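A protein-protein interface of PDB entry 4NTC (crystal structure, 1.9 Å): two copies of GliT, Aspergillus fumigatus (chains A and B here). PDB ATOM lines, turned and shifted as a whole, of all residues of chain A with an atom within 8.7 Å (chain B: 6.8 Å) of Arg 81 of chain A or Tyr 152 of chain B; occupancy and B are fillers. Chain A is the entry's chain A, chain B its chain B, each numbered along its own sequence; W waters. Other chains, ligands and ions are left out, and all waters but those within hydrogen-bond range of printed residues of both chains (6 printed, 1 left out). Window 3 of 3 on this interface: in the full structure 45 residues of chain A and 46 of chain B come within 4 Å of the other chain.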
ATOM      1  N   THR A  31      24.295 -10.415 -21.859  1.00  0.00           N
ATOM      2  CA  THR A  31      24.437  -9.365 -22.861  1.00  0.00           C
ATOM      3  C   THR A  31      25.367  -8.251 -22.372  1.00  0.00           C
ATOM      4  O   THR A  31      26.255  -7.814 -23.102  1.00  0.00           O
ATOM      5  CB  THR A  31      23.057  -8.797 -23.276  1.00  0.00           C
ATOM      6  OG1 THR A  31      22.262  -9.848 -23.830  1.00  0.00           O
ATOM      7  CG2 THR A  31      23.197  -7.685 -24.321  1.00  0.00           C
ATOM      8  N   GLY A  32      25.172  -7.812 -21.130  1.00  0.00           N
ATOM      9  CA  GLY A  32      26.015  -6.780 -20.535  1.00  0.00           C
ATOM     10  C   GLY A  32      27.448  -7.240 -20.344  1.00  0.00           C
ATOM     11  O   GLY A  32      28.384  -6.499 -20.641  1.00  0.00           O
ATOM     12  N   LEU A  33      27.619  -8.463 -19.847  1.00  0.00           N
ATOM     13  CA  LEU A  33      28.957  -9.026 -19.647  1.00  0.00           C
ATOM     14  C   LEU A  33      29.750  -9.144 -20.947  1.00  0.00           C
ATOM     15  O   LEU A  33      30.951  -8.853 -20.972  1.00  0.00           O
ATOM     16  CB  LEU A  33      28.878 -10.398 -18.976  1.00  0.00           C
ATOM     17  CG  LEU A  33      28.298 -10.485 -17.564  1.00  0.00           C
ATOM     18  CD1 LEU A  33      28.000 -11.939 -17.215  1.00  0.00           C
ATOM     19  CD2 LEU A  33      29.227  -9.850 -16.537  1.00  0.00           C
ATOM     20  N   ALA A  34      29.077  -9.567 -22.016  1.00  0.00           N
ATOM     21  CA  ALA A  34      29.702  -9.747 -23.328  1.00  0.00           C
ATOM     22  C   ALA A  34      30.309  -8.448 -23.865  1.00  0.00           C
ATOM     23  O   ALA A  34      31.344  -8.472 -24.534  1.00  0.00           O
ATOM     24  CB  ALA A  34      28.705 -10.319 -24.323  1.00  0.00           C
ATOM     25  N   ARG A  35      29.665  -7.321 -23.562  1.00  0.00           N
ATOM     26  CA  ARG A  35      30.150  -6.002 -23.992  1.00  0.00           C
ATOM     27  C   ARG A  35      31.543  -5.682 -23.467  1.00  0.00           C
ATOM     28  O   ARG A  35      32.297  -4.928 -24.097  1.00  0.00           O
ATOM     29  CB  ARG A  35      29.179  -4.904 -23.550  1.00  0.00           C
ATOM     30  CG  ARG A  35      27.824  -4.929 -24.254  1.00  0.00           C
ATOM     31  CD  ARG A  35      27.959  -4.787 -25.764  1.00  0.00           C
ATOM     32  NE  ARG A  35      28.557  -3.502 -26.148  1.00  0.00           N
ATOM     33  CZ  ARG A  35      29.042  -3.224 -27.355  1.00  0.00           C
ATOM     34  NH1 ARG A  35      29.008  -4.130 -28.325  1.00  0.00           N
ATOM     35  NH2 ARG A  35      29.556  -2.023 -27.598  1.00  0.00           N
ATOM     36  N   GLN A  36      31.870  -6.249 -22.309  1.00  0.00           N
ATOM     37  CA  GLN A  36      33.131  -5.987 -21.632  1.00  0.00           C
ATOM     38  C   GLN A  36      34.063  -7.207 -21.640  1.00  0.00           C
ATOM     39  O   GLN A  36      35.013  -7.285 -20.850  1.00  0.00           O
ATOM     40  CB  GLN A  36      32.856  -5.473 -20.215  1.00  0.00           C
ATOM     41  CG  GLN A  36      32.584  -3.975 -20.178  1.00  0.00           C
ATOM     42  CD  GLN A  36      33.865  -3.170 -20.118  1.00  0.00           C
ATOM     43  OE1 GLN A  36      34.289  -2.578 -21.112  1.00  0.00           O
ATOM     44  NE2 GLN A  36      34.499  -3.159 -18.950  1.00  0.00           N
ATOM     45  N   LEU A  37      33.784  -8.139 -22.553  1.00  0.00           N
ATOM     46  CA  LEU A  37      34.609  -9.343 -22.775  1.00  0.00           C
ATOM     47  C   LEU A  37      34.696 -10.285 -21.571  1.00  0.00           C
ATOM     48  O   LEU A  37      35.617 -11.106 -21.474  1.00  0.00           O
ATOM     49  CB  LEU A  37      36.009  -8.963 -23.285  1.00  0.00           C
ATOM     50  CG  LEU A  37      36.087  -8.501 -24.742  1.00  0.00           C
ATOM     51  CD1 LEU A  37      37.311  -7.619 -24.967  1.00  0.00           C
ATOM     52  CD2 LEU A  37      36.081  -9.697 -25.693  1.00  0.00           C
ATOM     53  N   HIS A  38      33.735 -10.170 -20.660  1.00  0.00           N
ATOM     54  CA  HIS A  38      33.699 -11.061 -19.511  1.00  0.00           C
ATOM     55  C   HIS A  38      33.066 -12.392 -19.872  1.00  0.00           C
ATOM     56  O   HIS A  38      32.170 -12.456 -20.713  1.00  0.00           O
ATOM     57  CB  HIS A  38      33.020 -10.403 -18.308  1.00  0.00           C
ATOM     58  CG  HIS A  38      33.868  -9.357 -17.652  1.00  0.00           C
ATOM     59  ND1 HIS A  38      34.965  -9.672 -16.882  1.00  0.00           N
ATOM     60  CD2 HIS A  38      33.806  -8.003 -17.685  1.00  0.00           C
ATOM     61  CE1 HIS A  38      35.534  -8.558 -16.453  1.00  0.00           C
ATOM     62  NE2 HIS A  38      34.847  -7.531 -16.923  1.00  0.00           N
ATOM     63  N   ARG A  75      20.008 -15.331 -27.755  1.00  0.00           N
ATOM     64  CA  ARG A  75      21.040 -16.364 -27.893  1.00  0.00           C
ATOM     65  C   ARG A  75      21.907 -16.146 -29.120  1.00  0.00           C
ATOM     66  O   ARG A  75      23.132 -16.279 -29.047  1.00  0.00           O
ATOM     67  CB  ARG A  75      20.412 -17.757 -27.961  1.00  0.00           C
ATOM     68  CG  ARG A  75      20.052 -18.327 -26.604  1.00  0.00           C
ATOM     69  CD  ARG A  75      19.235 -19.602 -26.730  1.00  0.00           C
ATOM     70  NE  ARG A  75      19.127 -20.278 -25.439  1.00  0.00           N
ATOM     71  CZ  ARG A  75      19.982 -21.197 -25.001  1.00  0.00           C
ATOM     72  NH1 ARG A  75      21.014 -21.569 -25.750  1.00  0.00           N
ATOM     73  NH2 ARG A  75      19.804 -21.751 -23.810  1.00  0.00           N
ATOM     74  N   ALA A  76      21.267 -15.824 -30.243  1.00  0.00           N
ATOM     75  CA  ALA A  76      21.975 -15.547 -31.488  1.00  0.00           C
ATOM     76  C   ALA A  76      22.890 -14.337 -31.324  1.00  0.00           C
ATOM     77  O   ALA A  76      24.062 -14.389 -31.696  1.00  0.00           O
ATOM     78  CB  ALA A  76      20.991 -15.327 -32.633  1.00  0.00           C
ATOM     79  N   ASP A  77      22.354 -13.265 -30.742  1.00  0.00           N
ATOM     80  CA  ASP A  77      23.124 -12.050 -30.470  1.00  0.00           C
ATOM     81  C   ASP A  77      24.314 -12.298 -29.550  1.00  0.00           C
ATOM     82  O   ASP A  77      25.311 -11.587 -29.634  1.00  0.00           O
ATOM     83  CB  ASP A  77      22.238 -10.958 -29.859  1.00  0.00           C
ATOM     84  CG  ASP A  77      21.304 -10.322 -30.872  1.00  0.00           C
ATOM     85  OD1 ASP A  77      21.434 -10.610 -32.078  1.00  0.00           O
ATOM     86  OD2 ASP A  77      20.435  -9.524 -30.462  1.00  0.00           O
ATOM     87  N   LEU A  78      24.208 -13.293 -28.673  1.00  0.00           N
ATOM     88  CA  LEU A  78      25.285 -13.580 -27.717  1.00  0.00           C
ATOM     89  C   LEU A  78      26.416 -14.437 -28.284  1.00  0.00           C
ATOM     90  O   LEU A  78      27.496 -14.493 -27.693  1.00  0.00           O
ATOM     91  CB  LEU A  78      24.733 -14.215 -26.431  1.00  0.00           C
ATOM     92  CG  LEU A  78      24.110 -13.237 -25.426  1.00  0.00           C
ATOM     93  CD1 LEU A  78      23.184 -13.955 -24.456  1.00  0.00           C
ATOM     94  CD2 LEU A  78      25.190 -12.475 -24.673  1.00  0.00           C
ATOM     95  N   THR A  79      26.181 -15.092 -29.420  1.00  0.00           N
ATOM     96  CA  THR A  79      27.177 -16.016 -29.987  1.00  0.00           C
ATOM     97  C   THR A  79      27.652 -15.595 -31.366  1.00  0.00           C
ATOM     98  O   THR A  79      28.624 -16.138 -31.894  1.00  0.00           O
ATOM     99  CB  THR A  79      26.631 -17.451 -30.080  1.00  0.00           C
ATOM    100  OG1 THR A  79      25.387 -17.442 -30.792  1.00  0.00           O
ATOM    101  CG2 THR A  79      26.411 -18.045 -28.688  1.00  0.00           C
ATOM    102  N   THR A  80      26.959 -14.633 -31.952  1.00  0.00           N
ATOM    103  CA  THR A  80      27.311 -14.188 -33.284  1.00  0.00           C
ATOM    104  C   THR A  80      28.501 -13.227 -33.270  1.00  0.00           C
ATOM    105  O   THR A  80      29.524 -13.524 -33.874  1.00  0.00           O
ATOM    106  CB  THR A  80      26.098 -13.577 -34.013  1.00  0.00           C
ATOM    107  OG1 THR A  80      25.029 -14.531 -34.031  1.00  0.00           O
ATOM    108  CG2 THR A  80      26.454 -13.228 -35.438  1.00  0.00           C
ATOM    109  N   ARG A  81      28.371 -12.092 -32.578  1.00  0.00           N
ATOM    110  CA  ARG A  81      29.432 -11.065 -32.545  1.00  0.00           C
ATOM    111  C   ARG A  81      30.300 -11.158 -31.283  1.00  0.00           C
ATOM    112  O   ARG A  81      31.252 -10.388 -31.115  1.00  0.00           O
ATOM    113  CB  ARG A  81      28.839  -9.650 -32.687  1.00  0.00           C
ATOM    114  CG  ARG A  81      28.270  -9.329 -34.065  1.00  0.00           C
ATOM    115  CD  ARG A  81      27.676  -7.924 -34.153  1.00  0.00           C
ATOM    116  NE  ARG A  81      28.699  -6.884 -34.043  1.00  0.00           N
ATOM    117  CZ  ARG A  81      28.908  -6.138 -32.961  1.00  0.00           C
ATOM    118  NH1 ARG A  81      28.160  -6.299 -31.872  1.00  0.00           N
ATOM    119  NH2 ARG A  81      29.874  -5.228 -32.967  1.00  0.00           N
ATOM    120  N   TYR A  82      29.966 -12.114 -30.411  1.00  0.00           N
ATOM    121  CA  TYR A  82      30.645 -12.302 -29.127  1.00  0.00           C
ATOM    122  C   TYR A  82      30.987 -13.763 -28.941  1.00  0.00           C
ATOM    123  O   TYR A  82      30.270 -14.639 -29.428  1.00  0.00           O
ATOM    124  CB  TYR A  82      29.761 -11.834 -27.962  1.00  0.00           C
ATOM    125  CG  TYR A  82      29.215 -10.436 -28.160  1.00  0.00           C
ATOM    126  CD1 TYR A  82      29.933  -9.318 -27.735  1.00  0.00           C
ATOM    127  CD2 TYR A  82      27.990 -10.231 -28.795  1.00  0.00           C
ATOM    128  CE1 TYR A  82      29.437  -8.034 -27.928  1.00  0.00           C
ATOM    129  CE2 TYR A  82      27.490  -8.954 -28.999  1.00  0.00           C
ATOM    130  CZ  TYR A  82      28.215  -7.860 -28.564  1.00  0.00           C
ATOM    131  OH  TYR A  82      27.721  -6.588 -28.762  1.00  0.00           O
ATOM    132  N   SER A  83      32.072 -14.031 -28.223  1.00  0.00           N
ATOM    133  CA  SER A  83      32.512 -15.408 -28.039  1.00  0.00           C
ATOM    134  C   SER A  83      32.912 -15.752 -26.608  1.00  0.00           C
ATOM    135  O   SER A  83      33.490 -16.816 -26.365  1.00  0.00           O
ATOM    136  CB  SER A  83      33.646 -15.733 -29.017  1.00  0.00           C
ATOM    137  OG  SER A  83      33.214 -15.612 -30.361  1.00  0.00           O
ATOM    138  N   THR A  84      32.585 -14.877 -25.657  1.00  0.00           N
ATOM    139  CA  THR A  84      32.928 -15.126 -24.255  1.00  0.00           C
ATOM    140  C   THR A  84      31.784 -15.778 -23.478  1.00  0.00           C
ATOM    141  O   THR A  84      31.962 -16.166 -22.327  1.00  0.00           O
ATOM    142  CB  THR A  84      33.394 -13.851 -23.526  1.00  0.00           C
ATOM    143  OG1 THR A  84      32.332 -12.893 -23.500  1.00  0.00           O
ATOM    144  CG2 THR A  84      34.627 -13.244 -24.213  1.00  0.00           C
ATOM    145  N   ILE A  85      30.623 -15.907 -24.117  1.00  0.00           N
ATOM    146  CA  ILE A  85      29.436 -16.437 -23.447  1.00  0.00           C
ATOM    147  C   ILE A  85      29.132 -17.867 -23.876  1.00  0.00           C
ATOM    148  O   ILE A  85      28.873 -18.137 -25.049  1.00  0.00           O
ATOM    149  CB  ILE A  85      28.191 -15.530 -23.650  1.00  0.00           C
ATOM    150  CG1 ILE A  85      28.496 -14.067 -23.272  1.00  0.00           C
ATOM    151  CG2 ILE A  85      26.990 -16.070 -22.874  1.00  0.00           C
ATOM    152  CD1 ILE A  85      28.988 -13.844 -21.849  1.00  0.00           C
ATOM    153  N   HIS B  55      24.558   1.995 -34.534  1.00  0.00           N
ATOM    154  CA  HIS B  55      24.487   0.678 -33.898  1.00  0.00           C
ATOM    155  C   HIS B  55      24.235   0.748 -32.400  1.00  0.00           C
ATOM    156  O   HIS B  55      25.038   1.296 -31.651  1.00  0.00           O
ATOM    157  CB  HIS B  55      25.765  -0.120 -34.195  1.00  0.00           C
ATOM    158  CG  HIS B  55      25.996  -0.358 -35.654  1.00  0.00           C
ATOM    159  ND1 HIS B  55      26.985   0.284 -36.369  1.00  0.00           N
ATOM    160  CD2 HIS B  55      25.350  -1.153 -36.539  1.00  0.00           C
ATOM    161  CE1 HIS B  55      26.943  -0.113 -37.629  1.00  0.00           C
ATOM    162  NE2 HIS B  55      25.958  -0.984 -37.758  1.00  0.00           N
ATOM    163  N   MET B  56      23.106   0.188 -31.979  1.00  0.00           N
ATOM    164  CA  MET B  56      22.708   0.126 -30.576  1.00  0.00           C
ATOM    165  C   MET B  56      23.231  -1.169 -29.961  1.00  0.00           C
ATOM    166  O   MET B  56      23.150  -2.221 -30.587  1.00  0.00           O
ATOM    167  CB  MET B  56      21.178   0.151 -30.498  1.00  0.00           C
ATOM    168  CG  MET B  56      20.593   0.273 -29.107  1.00  0.00           C
ATOM    169  SD  MET B  56      18.815   0.580 -29.194  1.00  0.00           S
ATOM    170  CE  MET B  56      18.210  -0.959 -29.879  1.00  0.00           C
ATOM    171  N   HIS B  57      23.764  -1.096 -28.743  1.00  0.00           N
ATOM    172  CA  HIS B  57      24.246  -2.296 -28.054  1.00  0.00           C
ATOM    173  C   HIS B  57      23.682  -2.383 -26.640  1.00  0.00           C
ATOM    174  O   HIS B  57      23.138  -1.404 -26.119  1.00  0.00           O
ATOM    175  CB  HIS B  57      25.784  -2.337 -28.036  1.00  0.00           C
ATOM    176  CG  HIS B  57      26.402  -2.221 -29.393  1.00  0.00           C
ATOM    177  ND1 HIS B  57      27.045  -1.078 -29.823  1.00  0.00           N
ATOM    178  CD2 HIS B  57      26.458  -3.098 -30.424  1.00  0.00           C
ATOM    179  CE1 HIS B  57      27.476  -1.261 -31.060  1.00  0.00           C
ATOM    180  NE2 HIS B  57      27.137  -2.479 -31.445  1.00  0.00           N
ATOM    181  N   ASP B  63      20.995  -6.439 -30.779  1.00  0.00           N
ATOM    182  CA  ASP B  63      22.438  -6.167 -30.902  1.00  0.00           C
ATOM    183  C   ASP B  63      22.820  -5.642 -32.279  1.00  0.00           C
ATOM    184  O   ASP B  63      22.490  -6.252 -33.302  1.00  0.00           O
ATOM    185  CB  ASP B  63      23.281  -7.408 -30.583  1.00  0.00           C
ATOM    186  CG  ASP B  63      24.777  -7.133 -30.685  1.00  0.00           C
ATOM    187  OD1 ASP B  63      25.297  -6.362 -29.851  1.00  0.00           O
ATOM    188  OD2 ASP B  63      25.431  -7.693 -31.595  1.00  0.00           O
ATOM    189  N   HIS B  64      23.521  -4.508 -32.288  1.00  0.00           N
ATOM    190  CA  HIS B  64      24.085  -3.920 -33.507  1.00  0.00           C
ATOM    191  C   HIS B  64      23.028  -3.336 -34.450  1.00  0.00           C
ATOM    192  O   HIS B  64      23.346  -2.941 -35.573  1.00  0.00           O
ATOM    193  CB  HIS B  64      25.007  -4.927 -34.231  1.00  0.00           C
ATOM    194  CG  HIS B  64      26.192  -4.295 -34.897  1.00  0.00           C
ATOM    195  ND1 HIS B  64      27.059  -3.455 -34.230  1.00  0.00           N
ATOM    196  CD2 HIS B  64      26.669  -4.399 -36.162  1.00  0.00           C
ATOM    197  CE1 HIS B  64      28.008  -3.054 -35.059  1.00  0.00           C
ATOM    198  NE2 HIS B  64      27.795  -3.613 -36.237  1.00  0.00           N
ATOM    199  N   LEU B 147      30.812   2.521 -22.121  1.00  0.00           N
ATOM    200  CA  LEU B 147      31.529   1.363 -22.648  1.00  0.00           C
ATOM    201  C   LEU B 147      30.689   0.070 -22.681  1.00  0.00           C
ATOM    202  O   LEU B 147      31.190  -0.994 -23.039  1.00  0.00           O
ATOM    203  CB  LEU B 147      32.887   1.184 -21.950  1.00  0.00           C
ATOM    204  CG  LEU B 147      33.898   2.325 -22.156  1.00  0.00           C
ATOM    205  CD1 LEU B 147      35.144   2.130 -21.310  1.00  0.00           C
ATOM    206  CD2 LEU B 147      34.274   2.495 -23.621  1.00  0.00           C
ATOM    207  N   PHE B 148      29.413   0.181 -22.319  1.00  0.00           N
ATOM    208  CA  PHE B 148      28.429  -0.845 -22.653  1.00  0.00           C
ATOM    209  C   PHE B 148      27.782  -0.527 -24.005  1.00  0.00           C
ATOM    210  O   PHE B 148      27.357  -1.427 -24.721  1.00  0.00           O
ATOM    211  CB  PHE B 148      27.366  -0.981 -21.556  1.00  0.00           C
ATOM    212  CG  PHE B 148      27.867  -1.635 -20.299  1.00  0.00           C
ATOM    213  CD1 PHE B 148      28.068  -3.009 -20.243  1.00  0.00           C
ATOM    214  CD2 PHE B 148      28.135  -0.879 -19.168  1.00  0.00           C
ATOM    215  CE1 PHE B 148      28.531  -3.614 -19.090  1.00  0.00           C
ATOM    216  CE2 PHE B 148      28.597  -1.481 -18.007  1.00  0.00           C
ATOM    217  CZ  PHE B 148      28.795  -2.849 -17.970  1.00  0.00           C
ATOM    218  N   CYS B 149      27.738   0.761 -24.345  1.00  0.00           N
ATOM    219  CA  CYS B 149      27.124   1.255 -25.580  1.00  0.00           C
ATOM    220  C   CYS B 149      28.048   1.127 -26.774  1.00  0.00           C
ATOM    221  O   CYS B 149      27.615   0.836 -27.887  1.00  0.00           O
ATOM    222  CB  CYS B 149      26.753   2.727 -25.421  1.00  0.00           C
ATOM    223  SG  CYS B 149      25.689   3.080 -24.008  1.00  0.00           S
ATOM    224  N   ASP B 150      29.325   1.375 -26.526  1.00  0.00           N
ATOM    225  CA  ASP B 150      30.339   1.383 -27.558  1.00  0.00           C
ATOM    226  C   ASP B 150      31.605   0.825 -26.936  1.00  0.00           C
ATOM    227  O   ASP B 150      31.569   0.295 -25.828  1.00  0.00           O
ATOM    228  CB  ASP B 150      30.586   2.815 -28.031  1.00  0.00           C
ATOM    229  CG  ASP B 150      29.431   3.370 -28.830  1.00  0.00           C
ATOM    230  OD1 ASP B 150      29.249   2.949 -29.995  1.00  0.00           O
ATOM    231  OD2 ASP B 150      28.709   4.237 -28.296  1.00  0.00           O
ATOM    232  N   GLY B 151      32.722   0.954 -27.638  1.00  0.00           N
ATOM    233  CA  GLY B 151      34.009   0.545 -27.090  1.00  0.00           C
ATOM    234  C   GLY B 151      34.421  -0.846 -27.521  1.00  0.00           C
ATOM    235  O   GLY B 151      35.536  -1.038 -28.004  1.00  0.00           O
ATOM    236  N   TYR B 152      33.526  -1.819 -27.339  1.00  0.00           N
ATOM    237  CA  TYR B 152      33.773  -3.198 -27.777  1.00  0.00           C
ATOM    238  C   TYR B 152      34.160  -3.262 -29.257  1.00  0.00           C
ATOM    239  O   TYR B 152      35.029  -4.037 -29.642  1.00  0.00           O
ATOM    240  CB  TYR B 152      32.544  -4.078 -27.519  1.00  0.00           C
ATOM    241  CG  TYR B 152      32.661  -5.506 -28.035  1.00  0.00           C
ATOM    242  CD1 TYR B 152      33.298  -6.493 -27.277  1.00  0.00           C
ATOM    243  CD2 TYR B 152      32.121  -5.872 -29.270  1.00  0.00           C
ATOM    244  CE1 TYR B 152      33.400  -7.799 -27.739  1.00  0.00           C
ATOM    245  CE2 TYR B 152      32.220  -7.178 -29.740  1.00  0.00           C
ATOM    246  CZ  TYR B 152      32.863  -8.134 -28.970  1.00  0.00           C
ATOM    247  OH  TYR B 152      32.965  -9.432 -29.419  1.00  0.00           O
ATOM    248  N   GLU B 153      33.499  -2.446 -30.080  1.00  0.00           N
ATOM    249  CA  GLU B 153      33.755  -2.399 -31.519  1.00  0.00           C
ATOM    250  C   GLU B 153      35.155  -1.887 -31.859  1.00  0.00           C
ATOM    251  O   GLU B 153      35.674  -2.175 -32.934  1.00  0.00           O
ATOM    252  CB  GLU B 153      32.701  -1.539 -32.231  1.00  0.00           C
ATOM    253  CG  GLU B 153      31.343  -2.213 -32.378  1.00  0.00           C
ATOM    254  CD  GLU B 153      30.646  -2.451 -31.050  1.00  0.00           C
ATOM    255  OE1 GLU B 153      30.762  -1.591 -30.151  1.00  0.00           O
ATOM    256  OE2 GLU B 153      29.978  -3.502 -30.907  1.00  0.00           O
ATOM    257  N   GLU B 154      35.756  -1.129 -30.944  1.00  0.00           N
ATOM    258  CA  GLU B 154      37.097  -0.583 -31.166  1.00  0.00           C
ATOM    259  C   GLU B 154      38.156  -1.225 -30.256  1.00  0.00           C
ATOM    260  O   GLU B 154      39.176  -0.609 -29.932  1.00  0.00           O
ATOM    261  CB  GLU B 154      37.081   0.945 -31.034  1.00  0.00           C
ATOM    262  CG  GLU B 154      36.493   1.663 -32.248  1.00  0.00           C
ATOM    263  CD  GLU B 154      37.237   1.378 -33.550  1.00  0.00           C
ATOM    264  OE1 GLU B 154      38.493   1.397 -33.560  1.00  0.00           O
ATOM    265  OE2 GLU B 154      36.556   1.146 -34.576  1.00  0.00           O
ATOM    266  N   ARG B 155      37.910  -2.474 -29.869  1.00  0.00           N
ATOM    267  CA  ARG B 155      38.792  -3.198 -28.952  1.00  0.00           C
ATOM    268  C   ARG B 155      40.136  -3.548 -29.593  1.00  0.00           C
ATOM    269  O   ARG B 155      40.257  -3.598 -30.818  1.00  0.00           O
ATOM    270  CB  ARG B 155      38.104  -4.468 -28.442  1.00  0.00           C
ATOM    271  CG  ARG B 155      37.893  -5.553 -29.490  1.00  0.00           C
ATOM    272  CD  ARG B 155      37.031  -6.662 -28.905  1.00  0.00           C
ATOM    273  NE  ARG B 155      36.713  -7.741 -29.845  1.00  0.00           N
ATOM    274  CZ  ARG B 155      35.783  -7.679 -30.796  1.00  0.00           C
ATOM    275  NH1 ARG B 155      35.073  -6.576 -30.979  1.00  0.00           N
ATOM    276  NH2 ARG B 155      35.569  -8.728 -31.575  1.00  0.00           N
ATOM    277  N   GLY B 156      41.141  -3.795 -28.758  1.00  0.00           N
ATOM    278  CA  GLY B 156      42.460  -4.175 -29.248  1.00  0.00           C
ATOM    279  C   GLY B 156      43.364  -2.981 -29.490  1.00  0.00           C
ATOM    280  O   GLY B 156      44.266  -3.039 -30.326  1.00  0.00           O
ATOM    281  N   LEU B 184      39.702  -3.048 -23.286  1.00  0.00           N
ATOM    282  CA  LEU B 184      39.710  -2.755 -24.716  1.00  0.00           C
ATOM    283  C   LEU B 184      41.072  -2.285 -25.221  1.00  0.00           C
ATOM    284  O   LEU B 184      41.261  -2.087 -26.426  1.00  0.00           O
ATOM    285  CB  LEU B 184      38.655  -1.680 -25.026  1.00  0.00           C
ATOM    286  CG  LEU B 184      37.266  -1.848 -24.397  1.00  0.00           C
ATOM    287  CD1 LEU B 184      36.456  -0.572 -24.545  1.00  0.00           C
ATOM    288  CD2 LEU B 184      36.520  -3.036 -25.001  1.00  0.00           C
ATOM    289  N   PHE B 249      41.055   5.939 -28.761  1.00  0.00           N
ATOM    290  CA  PHE B 249      39.836   6.730 -28.587  1.00  0.00           C
ATOM    291  C   PHE B 249      39.883   7.336 -27.191  1.00  0.00           C
ATOM    292  O   PHE B 249      40.760   6.992 -26.387  1.00  0.00           O
ATOM    293  CB  PHE B 249      38.547   5.903 -28.796  1.00  0.00           C
ATOM    294  CG  PHE B 249      38.469   4.633 -27.980  1.00  0.00           C
ATOM    295  CD1 PHE B 249      38.038   4.651 -26.653  1.00  0.00           C
ATOM    296  CD2 PHE B 249      38.775   3.405 -28.561  1.00  0.00           C
ATOM    297  CE1 PHE B 249      37.954   3.474 -25.915  1.00  0.00           C
ATOM    298  CE2 PHE B 249      38.688   2.227 -27.831  1.00  0.00           C
ATOM    299  CZ  PHE B 249      38.276   2.260 -26.509  1.00  0.00           C
HETATM  300  O   HOH W   1      32.766  -8.807 -33.038  1.00  0.00           O
HETATM  301  O   HOH W   2      25.906 -10.803 -32.158  1.00  0.00           O
HETATM  302  O   HOH W   3      33.805 -11.904 -27.585  1.00  0.00           O
HETATM  303  O   HOH W   4      20.776  -8.457 -33.816  1.00  0.00           O
HETATM  304  O   HOH W   5      33.174  -5.858 -33.035  1.00  0.00           O
HETATM  305  O   HOH W   6      24.796  -5.949 -27.111  1.00  0.00           O
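No position is printed for both chains.
The side-chain carboxylate (OD2) of Asp 77 of chain A lies within hydrogen-bond range of the backbone NH (N) of Asp 63 of chain B, at 3.2 Å.
O of Cys 149 of chain B is in hydrogen-bond range of NH2 of Arg 35 of chain A, at 3.5 Å.
NH2 of Arg 35 of chain A lies within hydrogen-bond range of ND1 of His 57 of chain B (3.5 Å).
O of Arg 81 of chain A lies within hydrogen-bond range of OH of Tyr 152 of chain B (2.6 Å).
The guanidinium group (NH1) of Arg 81 of chain A is in salt-bridge range of the side-chain carboxylate (OD2) of Asp 63 of chain B.
OD1 of Asp 63 of chain B lies within hydrogen-bond range of OH of Tyr 82 of chain A (2.7 Å).
The side-chain carboxylate (OE2) of Glu 153 of chain B is in salt-bridge range of the guanidinium group (NH2) of Arg 81 of chain A (2.7 Å).
The guanidinium group of Arg 35 of chain A is in hydrogen-bond range of the backbone carbonyl oxygen of Phe 148 of chain B, 2.8 Å away.
The guanidinium group of Arg 35 of chain A is in salt-bridge range of the side-chain carboxylate of Glu 153 of chain B (2.8 Å).
The guanidinium group of Arg 81 of chain A is in hydrogen-bond range of the side-chain hydroxyl of Tyr 82 of chain A (3.2 Å).
N of His 64 of chain B sits at hydrogen-bond distance from O of Met 56 of chain B, 2.9 Å away.
Water W6 lies within hydrogen-bond range of OD1 of Asp 63 of chain B (2.8 Å) and OH of Tyr 82 of chain A (3.4 Å).
Water W5 bridges NH1 of Arg 155 of chain B (2.9 Å) and NH2 of Arg 81 of chain A (3.4 Å).
Water W1 bridges the backbone carbonyl oxygen (O) of Arg 81 of chain A and the guanidinium group (NH2) of Arg 155 of chain B.
Hydrophobic or aromatic side chains of chain B within 4 Å of the printed part of chain A: His 57, His 64, Phe 148 and Tyr 152.
Printed residues of chain A that touch a printed residue of chain B: Gly 32, Ala 34, Arg 35, Gln 36, Leu 37, Asp 77, Arg 81 and Tyr 82.
Among the printed residues, 18 pairs touch across the chains.
Among the printed residues, Asp or Glu carboxylates within 4 Å of a Lys or Arg side-chain nitrogen of the other chain: Arg 35 of chain A with Glu 153 of chain B, Arg 81 of chain A with Asp 63 of chain B and Arg 81 of chain A with Glu 153 of chain B.
Of the printed residues of chain B, Asp 77 of chain A touches Asp 63 (3.2 Å).
Of chain B, only His 57, Asp 63, His 64, Tyr 152 and Glu 153 come within 4 Å of Arg 81 of chain A.
Of the printed residues of chain A, Cys 149 of chain B touches Arg 35 (3.5 Å).
No residue of chain A comes within 4 Å of Gly 151 of chain B.
Of chain A, only Ala 34, Arg 35, Leu 37, Arg 81 and Tyr 82 come within 4 Å of Tyr 152 of chain B.
Glu 153 of chain B touches just these residues of chain A: Arg 35 and Arg 81.
Arg 155 of chain B touches none of the printed residues of chain A.
The nearest residue of chain A that does not touch Tyr 152 of chain B is Ser 83 of chain A (4.8 Å).
The nearest printed residue of chain B that does not touch Ala 34 of chain A is Phe 148 of chain B (6.7 Å).
Ala 34 of chain A touches Tyr 152 of chain B (O to CE1, 3.9 Å).
Arg 35 of chain A touches Tyr 152 of chain B (O to CB, 3.5 Å).
Tyr 152 of chain B touches Leu 37 of chain A (CE1 to CD2, 3.9 Å).
Arg 81 of chain A touches His 57 of chain B.
CZ of Arg 81 of chain A touches ND1 of His 64 of chain B, at 3.5 Å.
Tyr 82 of chain A touches Tyr 152 of chain B.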
